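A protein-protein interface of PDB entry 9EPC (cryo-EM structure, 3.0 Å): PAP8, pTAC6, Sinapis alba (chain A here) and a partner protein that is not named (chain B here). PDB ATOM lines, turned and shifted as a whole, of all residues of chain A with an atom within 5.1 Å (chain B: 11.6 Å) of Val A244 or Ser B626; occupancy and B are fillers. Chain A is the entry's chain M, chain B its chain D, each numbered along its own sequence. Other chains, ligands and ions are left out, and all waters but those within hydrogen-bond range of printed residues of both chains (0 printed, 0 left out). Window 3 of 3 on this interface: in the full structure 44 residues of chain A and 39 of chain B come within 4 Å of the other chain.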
ATOM      1  N   LYS A 231     -21.444 -15.359 -16.210  1.00  0.00           N
ATOM      2  CA  LYS A 231     -22.630 -16.019 -16.738  1.00  0.00           C
ATOM      3  C   LYS A 231     -22.933 -15.542 -18.152  1.00  0.00           C
ATOM      4  O   LYS A 231     -22.917 -14.339 -18.430  1.00  0.00           O
ATOM      5  CB  LYS A 231     -23.827 -15.755 -15.828  1.00  0.00           C
ATOM      6  CG  LYS A 231     -25.163 -16.085 -16.462  1.00  0.00           C
ATOM      7  CD  LYS A 231     -26.315 -15.791 -15.523  1.00  0.00           C
ATOM      8  CE  LYS A 231     -27.645 -15.901 -16.243  1.00  0.00           C
ATOM      9  NZ  LYS A 231     -27.792 -17.212 -16.924  1.00  0.00           N
ATOM     10  N   HIS A 232     -23.208 -16.487 -19.045  1.00  0.00           N
ATOM     11  CA  HIS A 232     -23.661 -16.140 -20.385  1.00  0.00           C
ATOM     12  C   HIS A 232     -25.047 -15.516 -20.319  1.00  0.00           C
ATOM     13  O   HIS A 232     -25.909 -15.963 -19.559  1.00  0.00           O
ATOM     14  CB  HIS A 232     -23.692 -17.375 -21.281  1.00  0.00           C
ATOM     15  CG  HIS A 232     -22.355 -18.015 -21.486  1.00  0.00           C
ATOM     16  ND1 HIS A 232     -22.137 -18.984 -22.440  1.00  0.00           N
ATOM     17  CD2 HIS A 232     -21.170 -17.828 -20.860  1.00  0.00           C
ATOM     18  CE1 HIS A 232     -20.873 -19.366 -22.394  1.00  0.00           C
ATOM     19  NE2 HIS A 232     -20.264 -18.680 -21.444  1.00  0.00           N
ATOM     20  N   TYR A 233     -25.264 -14.480 -21.124  1.00  0.00           N
ATOM     21  CA  TYR A 233     -26.551 -13.796 -21.125  1.00  0.00           C
ATOM     22  C   TYR A 233     -27.631 -14.739 -21.640  1.00  0.00           C
ATOM     23  O   TYR A 233     -27.518 -15.279 -22.745  1.00  0.00           O
ATOM     24  CB  TYR A 233     -26.479 -12.535 -21.978  1.00  0.00           C
ATOM     25  CG  TYR A 233     -27.706 -11.662 -21.880  1.00  0.00           C
ATOM     26  CD1 TYR A 233     -27.979 -10.944 -20.725  1.00  0.00           C
ATOM     27  CD2 TYR A 233     -28.587 -11.548 -22.945  1.00  0.00           C
ATOM     28  CE1 TYR A 233     -29.099 -10.144 -20.630  1.00  0.00           C
ATOM     29  CE2 TYR A 233     -29.709 -10.748 -22.860  1.00  0.00           C
ATOM     30  CZ  TYR A 233     -29.958 -10.048 -21.701  1.00  0.00           C
ATOM     31  OH  TYR A 233     -31.075  -9.251 -21.611  1.00  0.00           O
ATOM     32  N   ARG A 236     -27.042 -18.378 -23.208  1.00  0.00           N
ATOM     33  CA  ARG A 236     -26.808 -18.687 -24.609  1.00  0.00           C
ATOM     34  C   ARG A 236     -25.446 -19.346 -24.793  1.00  0.00           C
ATOM     35  O   ARG A 236     -24.484 -19.054 -24.079  1.00  0.00           O
ATOM     36  CB  ARG A 236     -26.908 -17.426 -25.464  1.00  0.00           C
ATOM     37  CG  ARG A 236     -28.337 -16.983 -25.730  1.00  0.00           C
ATOM     38  CD  ARG A 236     -28.421 -16.047 -26.923  1.00  0.00           C
ATOM     39  NE  ARG A 236     -28.007 -14.689 -26.597  1.00  0.00           N
ATOM     40  CZ  ARG A 236     -28.844 -13.709 -26.287  1.00  0.00           C
ATOM     41  NH1 ARG A 236     -30.152 -13.904 -26.245  1.00  0.00           N
ATOM     42  NH2 ARG A 236     -28.358 -12.502 -26.015  1.00  0.00           N
ATOM     43  N   GLU A 242     -25.927 -14.870 -31.226  1.00  0.00           N
ATOM     44  CA  GLU A 242     -26.294 -13.813 -30.296  1.00  0.00           C
ATOM     45  C   GLU A 242     -25.612 -13.969 -28.942  1.00  0.00           C
ATOM     46  O   GLU A 242     -26.113 -13.449 -27.941  1.00  0.00           O
ATOM     47  CB  GLU A 242     -27.812 -13.770 -30.118  1.00  0.00           C
ATOM     48  CG  GLU A 242     -28.489 -12.594 -30.802  1.00  0.00           C
ATOM     49  CD  GLU A 242     -28.269 -11.285 -30.069  1.00  0.00           C
ATOM     50  OE1 GLU A 242     -27.787 -11.315 -28.918  1.00  0.00           O
ATOM     51  OE2 GLU A 242     -28.583 -10.220 -30.643  1.00  0.00           O
ATOM     52  N   PHE A 243     -24.489 -14.679 -28.890  1.00  0.00           N
ATOM     53  CA  PHE A 243     -23.790 -14.864 -27.627  1.00  0.00           C
ATOM     54  C   PHE A 243     -23.223 -13.544 -27.126  1.00  0.00           C
ATOM     55  O   PHE A 243     -22.681 -12.746 -27.896  1.00  0.00           O
ATOM     56  CB  PHE A 243     -22.662 -15.880 -27.772  1.00  0.00           C
ATOM     57  CG  PHE A 243     -21.667 -15.833 -26.648  1.00  0.00           C
ATOM     58  CD1 PHE A 243     -21.958 -16.407 -25.425  1.00  0.00           C
ATOM     59  CD2 PHE A 243     -20.447 -15.202 -26.811  1.00  0.00           C
ATOM     60  CE1 PHE A 243     -21.050 -16.358 -24.388  1.00  0.00           C
ATOM     61  CE2 PHE A 243     -19.535 -15.150 -25.778  1.00  0.00           C
ATOM     62  CZ  PHE A 243     -19.836 -15.727 -24.566  1.00  0.00           C
ATOM     63  N   VAL A 244     -23.342 -13.326 -25.821  1.00  0.00           N
ATOM     64  CA  VAL A 244     -22.772 -12.155 -25.170  1.00  0.00           C
ATOM     65  C   VAL A 244     -22.693 -12.454 -23.681  1.00  0.00           C
ATOM     66  O   VAL A 244     -23.559 -13.135 -23.126  1.00  0.00           O
ATOM     67  CB  VAL A 244     -23.600 -10.884 -25.473  1.00  0.00           C
ATOM     68  CG1 VAL A 244     -25.011 -11.017 -24.931  1.00  0.00           C
ATOM     69  CG2 VAL A 244     -22.916  -9.653 -24.913  1.00  0.00           C
ATOM     70  N   LEU A 245     -21.638 -11.963 -23.042  1.00  0.00           N
ATOM     71  CA  LEU A 245     -21.428 -12.229 -21.628  1.00  0.00           C
ATOM     72  C   LEU A 245     -22.248 -11.269 -20.779  1.00  0.00           C
ATOM     73  O   LEU A 245     -22.185 -10.049 -20.964  1.00  0.00           O
ATOM     74  CB  LEU A 245     -19.947 -12.113 -21.277  1.00  0.00           C
ATOM     75  CG  LEU A 245     -19.076 -13.270 -21.759  1.00  0.00           C
ATOM     76  CD1 LEU A 245     -17.640 -13.060 -21.339  1.00  0.00           C
ATOM     77  CD2 LEU A 245     -19.604 -14.579 -21.212  1.00  0.00           C
ATOM     78  N   ASP A 246     -23.021 -11.822 -19.848  1.00  0.00           N
ATOM     79  CA  ASP A 246     -23.802 -11.026 -18.904  1.00  0.00           C
ATOM     80  C   ASP A 246     -22.904 -10.710 -17.717  1.00  0.00           C
ATOM     81  O   ASP A 246     -22.747 -11.508 -16.795  1.00  0.00           O
ATOM     82  CB  ASP A 246     -25.062 -11.770 -18.481  1.00  0.00           C
ATOM     83  CG  ASP A 246     -25.826 -11.044 -17.396  1.00  0.00           C
ATOM     84  OD1 ASP A 246     -26.246  -9.892 -17.631  1.00  0.00           O
ATOM     85  OD2 ASP A 246     -26.011 -11.628 -16.308  1.00  0.00           O
ATOM     86  N   PHE A 247     -22.307  -9.520 -17.743  1.00  0.00           N
ATOM     87  CA  PHE A 247     -21.344  -9.132 -16.722  1.00  0.00           C
ATOM     88  C   PHE A 247     -21.988  -8.822 -15.379  1.00  0.00           C
ATOM     89  O   PHE A 247     -21.261  -8.617 -14.402  1.00  0.00           O
ATOM     90  CB  PHE A 247     -20.540  -7.927 -17.199  1.00  0.00           C
ATOM     91  CG  PHE A 247     -19.546  -8.253 -18.269  1.00  0.00           C
ATOM     92  CD1 PHE A 247     -18.899  -9.474 -18.277  1.00  0.00           C
ATOM     93  CD2 PHE A 247     -19.261  -7.344 -19.268  1.00  0.00           C
ATOM     94  CE1 PHE A 247     -17.984  -9.781 -19.258  1.00  0.00           C
ATOM     95  CE2 PHE A 247     -18.346  -7.646 -20.253  1.00  0.00           C
ATOM     96  CZ  PHE A 247     -17.708  -8.867 -20.247  1.00  0.00           C
ATOM     97  N   ARG A 277     -26.060  -5.231 -24.502  1.00  0.00           N
ATOM     98  CA  ARG A 277     -24.936  -5.902 -23.862  1.00  0.00           C
ATOM     99  C   ARG A 277     -23.681  -5.904 -24.723  1.00  0.00           C
ATOM    100  O   ARG A 277     -22.583  -6.096 -24.192  1.00  0.00           O
ATOM    101  CB  ARG A 277     -25.321  -7.339 -23.517  1.00  0.00           C
ATOM    102  CG  ARG A 277     -26.603  -7.461 -22.720  1.00  0.00           C
ATOM    103  CD  ARG A 277     -26.375  -7.150 -21.258  1.00  0.00           C
ATOM    104  NE  ARG A 277     -27.610  -7.250 -20.490  1.00  0.00           N
ATOM    105  CZ  ARG A 277     -27.659  -7.432 -19.179  1.00  0.00           C
ATOM    106  NH1 ARG A 277     -26.559  -7.565 -18.458  1.00  0.00           N
ATOM    107  NH2 ARG A 277     -28.843  -7.490 -18.577  1.00  0.00           N
ATOM    108  N   LYS A 278     -23.813  -5.696 -26.034  1.00  0.00           N
ATOM    109  CA  LYS A 278     -22.660  -5.776 -26.920  1.00  0.00           C
ATOM    110  C   LYS A 278     -21.652  -4.659 -26.680  1.00  0.00           C
ATOM    111  O   LYS A 278     -20.485  -4.807 -27.054  1.00  0.00           O
ATOM    112  CB  LYS A 278     -23.115  -5.756 -28.378  1.00  0.00           C
ATOM    113  CG  LYS A 278     -24.047  -6.895 -28.746  1.00  0.00           C
ATOM    114  CD  LYS A 278     -24.451  -6.824 -30.207  1.00  0.00           C
ATOM    115  CE  LYS A 278     -25.365  -7.976 -30.582  1.00  0.00           C
ATOM    116  NZ  LYS A 278     -25.787  -7.906 -32.007  1.00  0.00           N
ATOM    117  N   ASP A 279     -22.070  -3.551 -26.073  1.00  0.00           N
ATOM    118  CA  ASP A 279     -21.185  -2.425 -25.815  1.00  0.00           C
ATOM    119  C   ASP A 279     -20.608  -2.439 -24.406  1.00  0.00           C
ATOM    120  O   ASP A 279     -19.916  -1.492 -24.022  1.00  0.00           O
ATOM    121  CB  ASP A 279     -21.923  -1.110 -26.064  1.00  0.00           C
ATOM    122  CG  ASP A 279     -22.385  -0.968 -27.498  1.00  0.00           C
ATOM    123  OD1 ASP A 279     -21.739  -1.552 -28.392  1.00  0.00           O
ATOM    124  OD2 ASP A 279     -23.394  -0.271 -27.732  1.00  0.00           O
ATOM    125  N   ASP A 280     -20.878  -3.483 -23.629  1.00  0.00           N
ATOM    126  CA  ASP A 280     -20.358  -3.559 -22.273  1.00  0.00           C
ATOM    127  C   ASP A 280     -18.872  -3.890 -22.281  1.00  0.00           C
ATOM    128  O   ASP A 280     -18.357  -4.523 -23.206  1.00  0.00           O
ATOM    129  CB  ASP A 280     -21.121  -4.607 -21.468  1.00  0.00           C
ATOM    130  CG  ASP A 280     -22.592  -4.278 -21.333  1.00  0.00           C
ATOM    131  OD1 ASP A 280     -23.011  -3.217 -21.838  1.00  0.00           O
ATOM    132  OD2 ASP A 280     -23.328  -5.080 -20.722  1.00  0.00           O
ATOM    133  N   VAL B 622      -8.061  -5.450 -16.023  1.00  0.00           N
ATOM    134  CA  VAL B 622      -8.487  -6.437 -17.008  1.00  0.00           C
ATOM    135  C   VAL B 622      -9.670  -5.863 -17.771  1.00  0.00           C
ATOM    136  O   VAL B 622     -10.714  -5.570 -17.177  1.00  0.00           O
ATOM    137  CB  VAL B 622      -8.857  -7.774 -16.353  1.00  0.00           C
ATOM    138  CG1 VAL B 622      -9.301  -8.767 -17.406  1.00  0.00           C
ATOM    139  CG2 VAL B 622      -7.680  -8.317 -15.571  1.00  0.00           C
ATOM    140  N   HIS B 623      -9.510  -5.709 -19.081  1.00  0.00           N
ATOM    141  CA  HIS B 623     -10.565  -5.195 -19.951  1.00  0.00           C
ATOM    142  C   HIS B 623     -11.297  -6.388 -20.549  1.00  0.00           C
ATOM    143  O   HIS B 623     -10.871  -6.953 -21.557  1.00  0.00           O
ATOM    144  CB  HIS B 623      -9.986  -4.292 -21.031  1.00  0.00           C
ATOM    145  CG  HIS B 623      -9.379  -3.035 -20.500  1.00  0.00           C
ATOM    146  ND1 HIS B 623      -8.514  -2.256 -21.236  1.00  0.00           N
ATOM    147  CD2 HIS B 623      -9.513  -2.420 -19.302  1.00  0.00           C
ATOM    148  CE1 HIS B 623      -8.141  -1.215 -20.515  1.00  0.00           C
ATOM    149  NE2 HIS B 623      -8.732  -1.290 -19.337  1.00  0.00           N
ATOM    150  N   TYR B 624     -12.406  -6.762 -19.927  1.00  0.00           N
ATOM    151  CA  TYR B 624     -13.167  -7.950 -20.299  1.00  0.00           C
ATOM    152  C   TYR B 624     -14.286  -7.519 -21.241  1.00  0.00           C
ATOM    153  O   TYR B 624     -15.295  -6.959 -20.807  1.00  0.00           O
ATOM    154  CB  TYR B 624     -13.710  -8.629 -19.048  1.00  0.00           C
ATOM    155  CG  TYR B 624     -13.940 -10.113 -19.169  1.00  0.00           C
ATOM    156  CD1 TYR B 624     -14.171 -10.707 -20.399  1.00  0.00           C
ATOM    157  CD2 TYR B 624     -13.929 -10.922 -18.044  1.00  0.00           C
ATOM    158  CE1 TYR B 624     -14.382 -12.063 -20.502  1.00  0.00           C
ATOM    159  CE2 TYR B 624     -14.141 -12.275 -18.138  1.00  0.00           C
ATOM    160  CZ  TYR B 624     -14.367 -12.841 -19.368  1.00  0.00           C
ATOM    161  OH  TYR B 624     -14.577 -14.195 -19.460  1.00  0.00           O
ATOM    162  N   GLU B 625     -14.105  -7.776 -22.533  1.00  0.00           N
ATOM    163  CA  GLU B 625     -15.135  -7.442 -23.505  1.00  0.00           C
ATOM    164  C   GLU B 625     -16.291  -8.428 -23.417  1.00  0.00           C
ATOM    165  O   GLU B 625     -16.132  -9.571 -22.983  1.00  0.00           O
ATOM    166  CB  GLU B 625     -14.560  -7.435 -24.919  1.00  0.00           C
ATOM    167  CG  GLU B 625     -13.404  -6.473 -25.112  1.00  0.00           C
ATOM    168  CD  GLU B 625     -12.865  -6.487 -26.526  1.00  0.00           C
ATOM    169  OE1 GLU B 625     -13.515  -7.089 -27.406  1.00  0.00           O
ATOM    170  OE2 GLU B 625     -11.790  -5.898 -26.759  1.00  0.00           O
ATOM    171  N   SER B 626     -17.468  -7.974 -23.844  1.00  0.00           N
ATOM    172  CA  SER B 626     -18.673  -8.785 -23.732  1.00  0.00           C
ATOM    173  C   SER B 626     -18.692  -9.963 -24.694  1.00  0.00           C
ATOM    174  O   SER B 626     -19.556 -10.836 -24.553  1.00  0.00           O
ATOM    175  CB  SER B 626     -19.907  -7.916 -23.962  1.00  0.00           C
ATOM    176  OG  SER B 626     -19.875  -7.319 -25.245  1.00  0.00           O
ATOM    177  N   PHE B 627     -17.779 -10.015 -25.658  1.00  0.00           N
ATOM    178  CA  PHE B 627     -17.742 -11.100 -26.626  1.00  0.00           C
ATOM    179  C   PHE B 627     -16.797 -12.224 -26.232  1.00  0.00           C
ATOM    180  O   PHE B 627     -16.629 -13.171 -27.006  1.00  0.00           O
ATOM    181  CB  PHE B 627     -17.356 -10.562 -28.006  1.00  0.00           C
ATOM    182  CG  PHE B 627     -18.465  -9.828 -28.697  1.00  0.00           C
ATOM    183  CD1 PHE B 627     -19.783 -10.041 -28.332  1.00  0.00           C
ATOM    184  CD2 PHE B 627     -18.193  -8.928 -29.712  1.00  0.00           C
ATOM    185  CE1 PHE B 627     -20.808  -9.370 -28.965  1.00  0.00           C
ATOM    186  CE2 PHE B 627     -19.215  -8.254 -30.349  1.00  0.00           C
ATOM    187  CZ  PHE B 627     -20.525  -8.475 -29.975  1.00  0.00           C
ATOM    188  N   GLY B 628     -16.177 -12.147 -25.058  1.00  0.00           N
ATOM    189  CA  GLY B 628     -15.311 -13.193 -24.559  1.00  0.00           C
ATOM    190  C   GLY B 628     -13.839 -12.844 -24.562  1.00  0.00           C
ATOM    191  O   GLY B 628     -13.072 -13.457 -23.809  1.00  0.00           O
ATOM    192  N   ASN B 629     -13.420 -11.891 -25.386  1.00  0.00           N
ATOM    193  CA  ASN B 629     -12.031 -11.455 -25.367  1.00  0.00           C
ATOM    194  C   ASN B 629     -11.781 -10.578 -24.150  1.00  0.00           C
ATOM    195  O   ASN B 629     -12.537  -9.639 -23.887  1.00  0.00           O
ATOM    196  CB  ASN B 629     -11.697 -10.688 -26.641  1.00  0.00           C
ATOM    197  CG  ASN B 629     -11.889 -11.519 -27.885  1.00  0.00           C
ATOM    198  OD1 ASN B 629     -12.994 -11.617 -28.414  1.00  0.00           O
ATOM    199  ND2 ASN B 629     -10.808 -12.123 -28.363  1.00  0.00           N
ATOM    200  N   TYR B 630     -10.726 -10.881 -23.402  1.00  0.00           N
ATOM    201  CA  TYR B 630     -10.344 -10.058 -22.266  1.00  0.00           C
ATOM    202  C   TYR B 630      -8.852  -9.783 -22.314  1.00  0.00           C
ATOM    203  O   TYR B 630      -8.050 -10.703 -22.497  1.00  0.00           O
ATOM    204  CB  TYR B 630     -10.733 -10.707 -20.933  1.00  0.00           C
ATOM    205  CG  TYR B 630     -10.168 -12.083 -20.677  1.00  0.00           C
ATOM    206  CD1 TYR B 630     -10.789 -13.214 -21.182  1.00  0.00           C
ATOM    207  CD2 TYR B 630      -9.038 -12.252 -19.894  1.00  0.00           C
ATOM    208  CE1 TYR B 630     -10.286 -14.472 -20.935  1.00  0.00           C
ATOM    209  CE2 TYR B 630      -8.528 -13.506 -19.642  1.00  0.00           C
ATOM    210  CZ  TYR B 630      -9.157 -14.612 -20.164  1.00  0.00           C
ATOM    211  OH  TYR B 630      -8.650 -15.865 -19.916  1.00  0.00           O
ATOM    212  N   HIS B 631      -8.492  -8.515 -22.159  1.00  0.00           N
ATOM    213  CA  HIS B 631      -7.106  -8.084 -22.108  1.00  0.00           C
ATOM    214  C   HIS B 631      -6.682  -7.942 -20.657  1.00  0.00           C
ATOM    215  O   HIS B 631      -7.422  -7.397 -19.836  1.00  0.00           O
ATOM    216  CB  HIS B 631      -6.915  -6.750 -22.830  1.00  0.00           C
ATOM    217  CG  HIS B 631      -7.405  -6.748 -24.244  1.00  0.00           C
ATOM    218  ND1 HIS B 631      -8.717  -7.004 -24.579  1.00  0.00           N
ATOM    219  CD2 HIS B 631      -6.760  -6.510 -25.409  1.00  0.00           C
ATOM    220  CE1 HIS B 631      -8.857  -6.929 -25.890  1.00  0.00           C
ATOM    221  NE2 HIS B 631      -7.683  -6.631 -26.417  1.00  0.00           N
ATOM    222  N   ARG B 641      -6.225 -12.730 -23.928  1.00  0.00           N
ATOM    223  CA  ARG B 641      -6.850 -14.042 -23.949  1.00  0.00           C
ATOM    224  C   ARG B 641      -8.303 -13.917 -24.386  1.00  0.00           C
ATOM    225  O   ARG B 641      -8.860 -12.824 -24.484  1.00  0.00           O
ATOM    226  CB  ARG B 641      -6.762 -14.710 -22.576  1.00  0.00           C
ATOM    227  CG  ARG B 641      -5.350 -14.908 -22.074  1.00  0.00           C
ATOM    228  CD  ARG B 641      -5.269 -16.073 -21.105  1.00  0.00           C
ATOM    229  NE  ARG B 641      -5.956 -15.804 -19.851  1.00  0.00           N
ATOM    230  CZ  ARG B 641      -5.366 -15.315 -18.769  1.00  0.00           C
ATOM    231  NH1 ARG B 641      -4.078 -15.020 -18.760  1.00  0.00           N
ATOM    232  NH2 ARG B 641      -6.088 -15.119 -17.670  1.00  0.00           N
ATOM    233  N   SER B 642      -8.917 -15.064 -24.656  1.00  0.00           N
ATOM    234  CA  SER B 642     -10.306 -15.106 -25.078  1.00  0.00           C
ATOM    235  C   SER B 642     -10.979 -16.323 -24.467  1.00  0.00           C
ATOM    236  O   SER B 642     -10.325 -17.292 -24.079  1.00  0.00           O
ATOM    237  CB  SER B 642     -10.433 -15.142 -26.604  1.00  0.00           C
ATOM    238  OG  SER B 642     -11.793 -15.205 -26.994  1.00  0.00           O
ATOM    239  N   VAL B 643     -12.302 -16.254 -24.372  1.00  0.00           N
ATOM    240  CA  VAL B 643     -13.092 -17.385 -23.903  1.00  0.00           C
ATOM    241  C   VAL B 643     -13.436 -18.326 -25.046  1.00  0.00           C
ATOM    242  O   VAL B 643     -13.320 -19.547 -24.918  1.00  0.00           O
ATOM    243  CB  VAL B 643     -14.362 -16.883 -23.188  1.00  0.00           C
ATOM    244  CG1 VAL B 643     -15.313 -18.035 -22.935  1.00  0.00           C
ATOM    245  CG2 VAL B 643     -13.994 -16.201 -21.888  1.00  0.00           C
ATOM    246  N   LYS B 644     -13.860 -17.767 -26.181  1.00  0.00           N
ATOM    247  CA  LYS B 644     -14.172 -18.594 -27.340  1.00  0.00           C
ATOM    248  C   LYS B 644     -12.941 -19.341 -27.834  1.00  0.00           C
ATOM    249  O   LYS B 644     -13.022 -20.522 -28.191  1.00  0.00           O
ATOM    250  CB  LYS B 644     -14.749 -17.731 -28.461  1.00  0.00           C
ATOM    251  CG  LYS B 644     -16.138 -17.188 -28.191  1.00  0.00           C
ATOM    252  CD  LYS B 644     -16.596 -16.307 -29.341  1.00  0.00           C
ATOM    253  CE  LYS B 644     -18.083 -16.022 -29.267  1.00  0.00           C
ATOM    254  NZ  LYS B 644     -18.887 -17.266 -29.415  1.00  0.00           N
ATOM    255  N   LYS B 645     -11.795 -18.675 -27.855  1.00  0.00           N
ATOM    256  CA  LYS B 645     -10.573 -19.217 -28.427  1.00  0.00           C
ATOM    257  C   LYS B 645      -9.501 -19.331 -27.344  1.00  0.00           C
ATOM    258  O   LYS B 645      -9.757 -19.118 -26.158  1.00  0.00           O
ATOM    259  CB  LYS B 645     -10.112 -18.340 -29.592  1.00  0.00           C
ATOM    260  CG  LYS B 645     -11.199 -18.072 -30.619  1.00  0.00           C
ATOM    261  CD  LYS B 645     -10.859 -16.872 -31.485  1.00  0.00           C
ATOM    262  CE  LYS B 645     -10.791 -15.600 -30.655  1.00  0.00           C
ATOM    263  NZ  LYS B 645     -10.469 -14.407 -31.485  1.00  0.00           N
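No residue of chain B comes within 4 Å of His A232.
Val A244 touches just one residue of chain B: Ser B626 (3.5 Å).
No residue of chain B comes within 4 Å of Asp A246.
Of the printed residues of chain B, Phe A247 touches Tyr B624 (3.1 Å), Glu B625 (3.2 Å) and Ser B626 (3.6 Å).
Of chain B, only Ser B626 (3.2 Å) comes within 4 Å of Lys A278.
Of chain B, only Ser B626 comes within 4 Å of Asp A280.
Of the printed residues of chain A, Tyr B624 touches Leu A245 (3.5 Å) and Phe A247 (3.1 Å).
Of chain A, only Val A244 (3.5 Å), Leu A245 (2.8 Å), Phe A247 (3.6 Å), Arg A277 (3.2 Å), Lys A278 (3.2 Å) and Asp A280 (3.6 Å) come within 4 Å of Ser B626.
Lys B645 touches none of the printed residues of chain A.
The nearest residue of chain A that does not touch Ser B626 is Asp A279 (4.4 Å).
The nearest printed residue of chain B that does not touch Arg A277 is Phe B627 (6.1 Å).
Hydrophobic or aromatic side chains of chain A within 4 Å of the printed part of chain B: Phe A243, Val A244, Leu A245 and Phe A247.
Of the 15 printed residues of chain B, 6 touch a printed residue of chain A.
Hydrophobic or aromatic side chains of chain B that line the printed part of chain A: Tyr B624 and Phe B627.
Among the printed residues, no Asp or Glu carboxylate lies within 4 Å of a Lys or Arg side-chain nitrogen of the other chain.
N of Leu A245 lies within hydrogen-bond range of O of Ser B626 (2.8 Å).
OG of Ser B626 sits at hydrogen-bond distance from O of Arg A277, at 3.2 Å.
O of Lys A278 is in hydrogen-bond range of OG of Ser B626, at 3.2 Å.
The backbone NH of Tyr A233 sits at hydrogen-bond distance from the backbone carbonyl oxygen of Val A244 (3.0 Å).
OE2 of Glu A242 lies within salt-bridge range of NZ of Lys A278 (3.9 Å).
OD1 of Asp A246 lies within salt-bridge range of NH1 of Arg A277 (2.5 Å).
N of Val B643 is in hydrogen-bond range of O of Gly B628 (3.0 Å).
N of Lys B644 sits at hydrogen-bond distance from OG of Ser B642 (3.4 Å).
Among the printed residues, merely in contact across the chains: Phe A243 with Phe B627 (3.7 Å), Phe A243 with Lys B644 (3.5 Å), Val A244 with Ser B626 (3.5 Å), Leu A245 with Tyr B624 (3.5 Å), Leu A245 with Gly B628 (3.98 Å), Phe A247 with Tyr B624 (3.1 Å), Phe A247 with Glu B625 (3.2 Å), Phe A247 with Ser B626 (3.6 Å) and Asp A280 with Ser B626 (3.6 Å).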
